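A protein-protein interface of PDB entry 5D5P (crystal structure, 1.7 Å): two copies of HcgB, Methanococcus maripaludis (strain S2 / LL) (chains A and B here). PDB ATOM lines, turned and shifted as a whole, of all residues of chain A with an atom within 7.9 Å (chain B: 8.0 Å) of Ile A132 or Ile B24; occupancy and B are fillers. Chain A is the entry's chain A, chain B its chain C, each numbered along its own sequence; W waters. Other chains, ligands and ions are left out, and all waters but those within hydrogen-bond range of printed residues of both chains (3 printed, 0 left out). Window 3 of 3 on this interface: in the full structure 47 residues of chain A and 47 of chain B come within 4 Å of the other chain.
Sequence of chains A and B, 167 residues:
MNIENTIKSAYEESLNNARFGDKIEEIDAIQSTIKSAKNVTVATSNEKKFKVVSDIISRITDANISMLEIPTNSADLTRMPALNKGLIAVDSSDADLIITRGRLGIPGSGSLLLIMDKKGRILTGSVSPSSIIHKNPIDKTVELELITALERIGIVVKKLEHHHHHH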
ATOM      1  N   GLY A 108     -23.848   5.979  -2.825  1.00  0.00           N
ATOM      2  CA  GLY A 108     -24.294   5.404  -4.085  1.00  0.00           C
ATOM      3  C   GLY A 108     -25.721   5.796  -4.431  1.00  0.00           C
ATOM      4  O   GLY A 108     -26.149   5.599  -5.576  1.00  0.00           O
ATOM      5  N   PRO A 129     -28.751  11.238 -10.493  1.00  0.00           N
ATOM      6  CA  PRO A 129     -28.020   9.985 -10.274  1.00  0.00           C
ATOM      7  C   PRO A 129     -26.600  10.221  -9.785  1.00  0.00           C
ATOM      8  O   PRO A 129     -26.021  11.272 -10.063  1.00  0.00           O
ATOM      9  CB  PRO A 129     -27.988   9.334 -11.656  1.00  0.00           C
ATOM     10  CG  PRO A 129     -29.027  10.073 -12.467  1.00  0.00           C
ATOM     11  CD  PRO A 129     -29.066  11.455 -11.919  1.00  0.00           C
ATOM     12  N   SER A 130     -26.051   9.218  -9.099  1.00  0.00           N
ATOM     13  CA  SER A 130     -24.629   9.168  -8.815  1.00  0.00           C
ATOM     14  C   SER A 130     -23.783   9.421 -10.075  1.00  0.00           C
ATOM     15  O   SER A 130     -24.155   9.046 -11.176  1.00  0.00           O
ATOM     16  CB  SER A 130     -24.272   7.793  -8.237  1.00  0.00           C
ATOM     17  OG  SER A 130     -22.882   7.559  -8.338  1.00  0.00           O
ATOM     18  N   SER A 131     -22.612  10.023  -9.909  1.00  0.00           N
ATOM     19  CA  SER A 131     -21.743  10.204 -11.051  1.00  0.00           C
ATOM     20  C   SER A 131     -21.268   8.869 -11.633  1.00  0.00           C
ATOM     21  O   SER A 131     -20.888   8.804 -12.782  1.00  0.00           O
ATOM     22  CB  SER A 131     -20.547  11.066 -10.657  1.00  0.00           C
ATOM     23  OG  SER A 131     -19.837  10.456  -9.595  1.00  0.00           O
ATOM     24  N   ILE A 132     -21.329   7.799 -10.848  1.00  0.00           N
ATOM     25  CA  ILE A 132     -20.974   6.469 -11.341  1.00  0.00           C
ATOM     26  C   ILE A 132     -21.922   6.022 -12.458  1.00  0.00           C
ATOM     27  O   ILE A 132     -21.539   5.331 -13.398  1.00  0.00           O
ATOM     28  CB  ILE A 132     -21.037   5.423 -10.182  1.00  0.00           C
ATOM     29  CG1 ILE A 132     -19.978   5.731  -9.124  1.00  0.00           C
ATOM     30  CG2 ILE A 132     -20.865   3.988 -10.705  1.00  0.00           C
ATOM     31  CD1 ILE A 132     -18.600   5.353  -9.574  1.00  0.00           C
ATOM     32  N   ILE A 133     -23.180   6.416 -12.314  1.00  0.00           N
ATOM     33  CA  ILE A 133     -24.247   6.005 -13.217  1.00  0.00           C
ATOM     34  C   ILE A 133     -24.377   6.948 -14.410  1.00  0.00           C
ATOM     35  O   ILE A 133     -24.582   6.510 -15.531  1.00  0.00           O
ATOM     36  CB  ILE A 133     -25.588   5.950 -12.458  1.00  0.00           C
ATOM     37  CG1 ILE A 133     -25.527   4.892 -11.341  1.00  0.00           C
ATOM     38  CG2 ILE A 133     -26.758   5.685 -13.393  1.00  0.00           C
ATOM     39  CD1 ILE A 133     -25.268   3.495 -11.856  1.00  0.00           C
ATOM     40  N   HIS A 134     -24.292   8.246 -14.145  1.00  0.00           N
ATOM     41  CA  HIS A 134     -24.446   9.242 -15.196  1.00  0.00           C
ATOM     42  C   HIS A 134     -23.382  10.328 -15.085  1.00  0.00           C
ATOM     43  O   HIS A 134     -23.336  11.065 -14.092  1.00  0.00           O
ATOM     44  CB  HIS A 134     -25.835   9.863 -15.139  1.00  0.00           C
ATOM     45  CG  HIS A 134     -26.095  10.840 -16.244  1.00  0.00           C
ATOM     46  ND1 HIS A 134     -26.309  12.184 -16.018  1.00  0.00           N
ATOM     47  CD2 HIS A 134     -26.147  10.668 -17.588  1.00  0.00           C
ATOM     48  CE1 HIS A 134     -26.502  12.794 -17.178  1.00  0.00           C
ATOM     49  NE2 HIS A 134     -26.409  11.897 -18.143  1.00  0.00           N
ATOM     50  N   LYS A 135     -22.548  10.420 -16.113  1.00  0.00           N
ATOM     51  CA  LYS A 135     -21.482  11.408 -16.200  1.00  0.00           C
ATOM     52  C   LYS A 135     -22.042  12.714 -16.737  1.00  0.00           C
ATOM     53  O   LYS A 135     -22.655  12.745 -17.810  1.00  0.00           O
ATOM     54  CB  LYS A 135     -20.374  10.951 -17.153  1.00  0.00           C
ATOM     55  CG  LYS A 135     -19.678   9.614 -16.915  1.00  0.00           C
ATOM     56  CD  LYS A 135     -19.212   9.407 -15.488  1.00  0.00           C
ATOM     57  CE  LYS A 135     -19.314   7.935 -15.090  1.00  0.00           C
ATOM     58  NZ  LYS A 135     -18.351   7.625 -13.988  1.00  0.00           N
ATOM     59  N   THR B   6     -19.864  -0.765   2.701  1.00  0.00           N
ATOM     60  CA  THR B   6     -19.713   0.447   1.917  1.00  0.00           C
ATOM     61  C   THR B   6     -20.000   1.646   2.788  1.00  0.00           C
ATOM     62  O   THR B   6     -19.383   2.692   2.629  1.00  0.00           O
ATOM     63  CB  THR B   6     -20.622   0.447   0.653  1.00  0.00           C
ATOM     64  OG1 THR B   6     -22.007   0.452   1.032  1.00  0.00           O
ATOM     65  CG2 THR B   6     -20.320  -0.770  -0.170  1.00  0.00           C
ATOM     66  N   GLY B  21     -15.645  11.380  -4.211  1.00  0.00           N
ATOM     67  CA  GLY B  21     -16.662  10.896  -5.134  1.00  0.00           C
ATOM     68  C   GLY B  21     -17.255   9.573  -4.703  1.00  0.00           C
ATOM     69  O   GLY B  21     -16.774   8.951  -3.761  1.00  0.00           O
ATOM     70  N   ASP B  22     -18.317   9.138  -5.384  1.00  0.00           N
ATOM     71  CA  ASP B  22     -18.809   7.787  -5.183  1.00  0.00           C
ATOM     72  C   ASP B  22     -17.914   6.723  -5.813  1.00  0.00           C
ATOM     73  O   ASP B  22     -16.979   7.003  -6.595  1.00  0.00           O
ATOM     74  CB  ASP B  22     -20.217   7.603  -5.741  1.00  0.00           C
ATOM     75  CG  ASP B  22     -21.204   8.593  -5.188  1.00  0.00           C
ATOM     76  OD1 ASP B  22     -20.859   9.312  -4.221  1.00  0.00           O
ATOM     77  OD2 ASP B  22     -22.342   8.624  -5.718  1.00  0.00           O
ATOM     78  N   LYS B  23     -18.219   5.486  -5.439  1.00  0.00           N
ATOM     79  CA  LYS B  23     -17.431   4.345  -5.854  1.00  0.00           C
ATOM     80  C   LYS B  23     -18.336   3.315  -6.505  1.00  0.00           C
ATOM     81  O   LYS B  23     -19.489   3.163  -6.132  1.00  0.00           O
ATOM     82  CB  LYS B  23     -16.709   3.745  -4.651  1.00  0.00           C
ATOM     83  CG  LYS B  23     -15.810   4.740  -3.912  1.00  0.00           C
ATOM     84  CD  LYS B  23     -14.809   4.044  -3.012  1.00  0.00           C
ATOM     85  CE  LYS B  23     -13.703   4.998  -2.587  1.00  0.00           C
ATOM     86  NZ  LYS B  23     -12.984   4.486  -1.374  1.00  0.00           N
ATOM     87  N   ILE B  24     -17.783   2.572  -7.452  1.00  0.00           N
ATOM     88  CA  ILE B  24     -18.553   1.536  -8.131  1.00  0.00           C
ATOM     89  C   ILE B  24     -19.073   0.461  -7.167  1.00  0.00           C
ATOM     90  O   ILE B  24     -20.154  -0.077  -7.368  1.00  0.00           O
ATOM     91  CB  ILE B  24     -17.659   0.900  -9.248  1.00  0.00           C
ATOM     92  CG1 ILE B  24     -18.393  -0.189 -10.013  1.00  0.00           C
ATOM     93  CG2 ILE B  24     -16.388   0.322  -8.652  1.00  0.00           C
ATOM     94  CD1 ILE B  24     -19.701   0.287 -10.644  1.00  0.00           C
ATOM     95  N   GLU B  25     -18.300   0.173  -6.112  1.00  0.00           N
ATOM     96  CA  GLU B  25     -18.691  -0.783  -5.082  1.00  0.00           C
ATOM     97  C   GLU B  25     -19.993  -0.406  -4.412  1.00  0.00           C
ATOM     98  O   GLU B  25     -20.750  -1.272  -3.947  1.00  0.00           O
ATOM     99  CB  GLU B  25     -17.634  -0.899  -3.991  1.00  0.00           C
ATOM    100  CG  GLU B  25     -16.325  -1.521  -4.396  1.00  0.00           C
ATOM    101  CD  GLU B  25     -15.302  -0.495  -4.814  1.00  0.00           C
ATOM    102  OE1 GLU B  25     -14.151  -0.571  -4.326  1.00  0.00           O
ATOM    103  OE2 GLU B  25     -15.685   0.485  -5.479  1.00  0.00           O
ATOM    104  N   GLU B  26     -20.229   0.896  -4.305  1.00  0.00           N
ATOM    105  CA  GLU B  26     -21.417   1.383  -3.618  1.00  0.00           C
ATOM    106  C   GLU B  26     -22.652   1.115  -4.447  1.00  0.00           C
ATOM    107  O   GLU B  26     -23.692   0.724  -3.915  1.00  0.00           O
ATOM    108  CB  GLU B  26     -21.263   2.877  -3.301  1.00  0.00           C
ATOM    109  CG  GLU B  26     -20.110   3.078  -2.292  1.00  0.00           C
ATOM    110  CD  GLU B  26     -19.611   4.494  -2.239  1.00  0.00           C
ATOM    111  OE1 GLU B  26     -20.089   5.316  -3.052  1.00  0.00           O
ATOM    112  OE2 GLU B  26     -18.737   4.788  -1.387  1.00  0.00           O
ATOM    113  N   ILE B  27     -22.535   1.298  -5.755  1.00  0.00           N
ATOM    114  CA  ILE B  27     -23.626   0.971  -6.649  1.00  0.00           C
ATOM    115  C   ILE B  27     -23.860  -0.546  -6.651  1.00  0.00           C
ATOM    116  O   ILE B  27     -25.014  -1.007  -6.553  1.00  0.00           O
ATOM    117  CB  ILE B  27     -23.350   1.491  -8.081  1.00  0.00           C
ATOM    118  CG1 ILE B  27     -23.490   3.021  -8.075  1.00  0.00           C
ATOM    119  CG2 ILE B  27     -24.311   0.879  -9.071  1.00  0.00           C
ATOM    120  CD1 ILE B  27     -24.876   3.494  -7.765  1.00  0.00           C
ATOM    121  N   ASP B  28     -22.770  -1.310  -6.716  1.00  0.00           N
ATOM    122  CA  ASP B  28     -22.854  -2.772  -6.697  1.00  0.00           C
ATOM    123  C   ASP B  28     -23.585  -3.268  -5.451  1.00  0.00           C
ATOM    124  O   ASP B  28     -24.441  -4.149  -5.540  1.00  0.00           O
ATOM    125  CB  ASP B  28     -21.461  -3.401  -6.742  1.00  0.00           C
ATOM    126  CG  ASP B  28     -20.818  -3.328  -8.129  1.00  0.00           C
ATOM    127  OD1 ASP B  28     -21.519  -3.036  -9.127  1.00  0.00           O
ATOM    128  OD2 ASP B  28     -19.592  -3.562  -8.216  1.00  0.00           O
ATOM    129  N   ALA B  29     -23.280  -2.685  -4.287  1.00  0.00           N
ATOM    130  CA  ALA B  29     -23.945  -3.104  -3.055  1.00  0.00           C
ATOM    131  C   ALA B  29     -25.453  -2.817  -3.078  1.00  0.00           C
ATOM    132  O   ALA B  29     -26.255  -3.631  -2.614  1.00  0.00           O
ATOM    133  CB  ALA B  29     -23.294  -2.414  -1.829  1.00  0.00           C
ATOM    134  N   ILE B  30     -25.829  -1.659  -3.609  1.00  0.00           N
ATOM    135  CA  ILE B  30     -27.238  -1.318  -3.732  1.00  0.00           C
ATOM    136  C   ILE B  30     -27.969  -2.306  -4.645  1.00  0.00           C
ATOM    137  O   ILE B  30     -29.034  -2.812  -4.286  1.00  0.00           O
ATOM    138  CB  ILE B  30     -27.434   0.127  -4.260  1.00  0.00           C
ATOM    139  CG1 ILE B  30     -27.035   1.138  -3.166  1.00  0.00           C
ATOM    140  CG2 ILE B  30     -28.897   0.352  -4.624  1.00  0.00           C
ATOM    141  CD1 ILE B  30     -26.934   2.590  -3.658  1.00  0.00           C
ATOM    142  N   GLN B  31     -27.391  -2.600  -5.810  1.00  0.00           N
ATOM    143  CA  GLN B  31     -28.047  -3.500  -6.744  1.00  0.00           C
ATOM    144  C   GLN B  31     -28.188  -4.892  -6.160  1.00  0.00           C
ATOM    145  O   GLN B  31     -29.249  -5.530  -6.306  1.00  0.00           O
ATOM    146  CB  GLN B  31     -27.297  -3.566  -8.072  1.00  0.00           C
ATOM    147  CG  GLN B  31     -27.317  -2.256  -8.817  1.00  0.00           C
ATOM    148  CD  GLN B  31     -26.668  -2.390 -10.170  1.00  0.00           C
ATOM    149  OE1 GLN B  31     -26.254  -3.489 -10.556  1.00  0.00           O
ATOM    150  NE2 GLN B  31     -26.578  -1.286 -10.908  1.00  0.00           N
ATOM    151  N   ARG B 152     -31.527   5.082 -11.834  1.00  0.00           N
ATOM    152  CA  ARG B 152     -30.468   5.957 -11.327  1.00  0.00           C
ATOM    153  C   ARG B 152     -29.486   5.211 -10.435  1.00  0.00           C
ATOM    154  O   ARG B 152     -28.434   5.749 -10.095  1.00  0.00           O
ATOM    155  CB  ARG B 152     -31.061   7.173 -10.595  1.00  0.00           C
ATOM    156  CG  ARG B 152     -31.851   6.846  -9.400  1.00  0.00           C
ATOM    157  CD  ARG B 152     -32.646   8.069  -8.935  1.00  0.00           C
ATOM    158  NE  ARG B 152     -31.809   9.119  -8.351  1.00  0.00           N
ATOM    159  CZ  ARG B 152     -31.229   9.023  -7.149  1.00  0.00           C
ATOM    160  NH1 ARG B 152     -31.348   7.911  -6.433  1.00  0.00           N
ATOM    161  NH2 ARG B 152     -30.494  10.040  -6.686  1.00  0.00           N
ATOM    162  N   ILE B 153     -29.786   3.962 -10.082  1.00  0.00           N
ATOM    163  CA  ILE B 153     -28.737   3.155  -9.462  1.00  0.00           C
ATOM    164  C   ILE B 153     -28.324   2.004 -10.379  1.00  0.00           C
ATOM    165  O   ILE B 153     -27.727   1.028  -9.937  1.00  0.00           O
ATOM    166  CB  ILE B 153     -29.145   2.657  -8.054  1.00  0.00           C
ATOM    167  CG1 ILE B 153     -30.544   2.033  -8.034  1.00  0.00           C
ATOM    168  CG2 ILE B 153     -29.103   3.835  -7.026  1.00  0.00           C
ATOM    169  CD1 ILE B 153     -30.594   0.634  -8.581  1.00  0.00           C
ATOM    170  N   GLY B 154     -28.624   2.131 -11.677  1.00  0.00           N
ATOM    171  CA  GLY B 154     -28.046   1.229 -12.652  1.00  0.00           C
ATOM    172  C   GLY B 154     -28.833  -0.029 -12.967  1.00  0.00           C
ATOM    173  O   GLY B 154     -28.308  -0.940 -13.599  1.00  0.00           O
HETATM  174  O   HOH W   1     -22.226  11.458  -7.382  1.00  0.00           O
HETATM  175  O   HOH W   2     -27.544   7.074  -7.894  1.00  0.00           O
HETATM  176  O   HOH W   3     -24.192   8.675  -4.189  1.00  0.00           O
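OG of Ser A130 sits at hydrogen-bond distance from OD2 of Asp B22, at 2.9 Å.
NE2 of Gln B31 sits at hydrogen-bond distance from O of Ile B153, 2.8 Å away.
The side-chain hydroxyl (OG) of Ser A130 is in hydrogen-bond range of the backbone NH (N) of Ile A132, at 3.0 Å.
The side-chain amide nitrogen of Gln B31 lies within hydrogen-bond range of the backbone carbonyl oxygen of Gly B154 (3.2 Å).
The backbone NH of Lys B23 sits at hydrogen-bond distance from the side-chain carboxylate of Glu B26, 3.0 Å away.
Glu B26 touches Gly A108 (OE1 to N, 3.8 Å).
Ile B27 touches Gly A108 (CD1 to O, 3.3 Å).
CB of Pro A129 touches CB of Arg B152 (3.9 Å).
Asp B22 touches Ile A132.
C of Lys B23 touches CD1 of Ile A132, at 3.7 Å.
Ile B27 touches Ile A132 (CG1 to CG2, 3.8 Å).
CG1 of Ile A133 touches CD1 of Ile B27, at 3.9 Å.
CG1 of Ile A133 touches O of Arg B152, at 3.3 Å.
Ile A133 touches Ile B153 (CD1 to C, 3.7 Å).
CD1 of Ile A133 touches N of Gly B154, at 3.6 Å.
Ile A132 touches just these residues of chain B: Asp B22 (3.8 Å), Lys B23 (3.7 Å), Ile B24 (3.6 Å) and Ile B27 (3.8 Å).
Of chain A, only Ile A132 (3.6 Å) comes within 4 Å of Ile B24.
No residue of chain B comes within 4 Å of Ser A131.
Of the printed residues of chain A, Lys B23 touches Ile A132 (3.7 Å).
Printed residues of chain B within 4 Å of Ile A133: Ile B27, Arg B152, Ile B153 and Gly B154.
Of the printed residues of chain A, Glu B26 touches Gly A108 (3.8 Å).
Of the printed residues of chain A, Gly B154 touches Ile A133 (3.6 Å).
The nearest residue of chain A that does not touch Ile B24 is Ile A133 (6.5 Å).
Printed residues of chain B that touch a printed residue of chain A: Asp B22, Lys B23, Ile B24, Glu B26, Ile B27, Ile B30, Arg B152, Ile B153 and Gly B154.
Of the 8 printed residues of chain A, 5 touch a printed residue of chain B.
Printed residues of chain A that touch a printed residue of chain B: Gly A108, Pro A129, Ser A130, Ile A132 and Ile A133.
No position is printed for both chains.
Of the 14 pairs that touch across the chains among the printed residues, none has its exchanged pair printed and touching as well.
Water W3 bridges the side-chain carboxylate of Asp B22 and the backbone NH of Gly A108.
Water W2 lies within hydrogen-bond range of the backbone carbonyl oxygen of Arg B152, the backbone NH of Ser A130 and the backbone carbonyl oxygen of Gly A108.
Water W1 lies within hydrogen-bond range of N of Ser A131 (2.9 Å) and OD2 of Asp B22 (3.3 Å).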
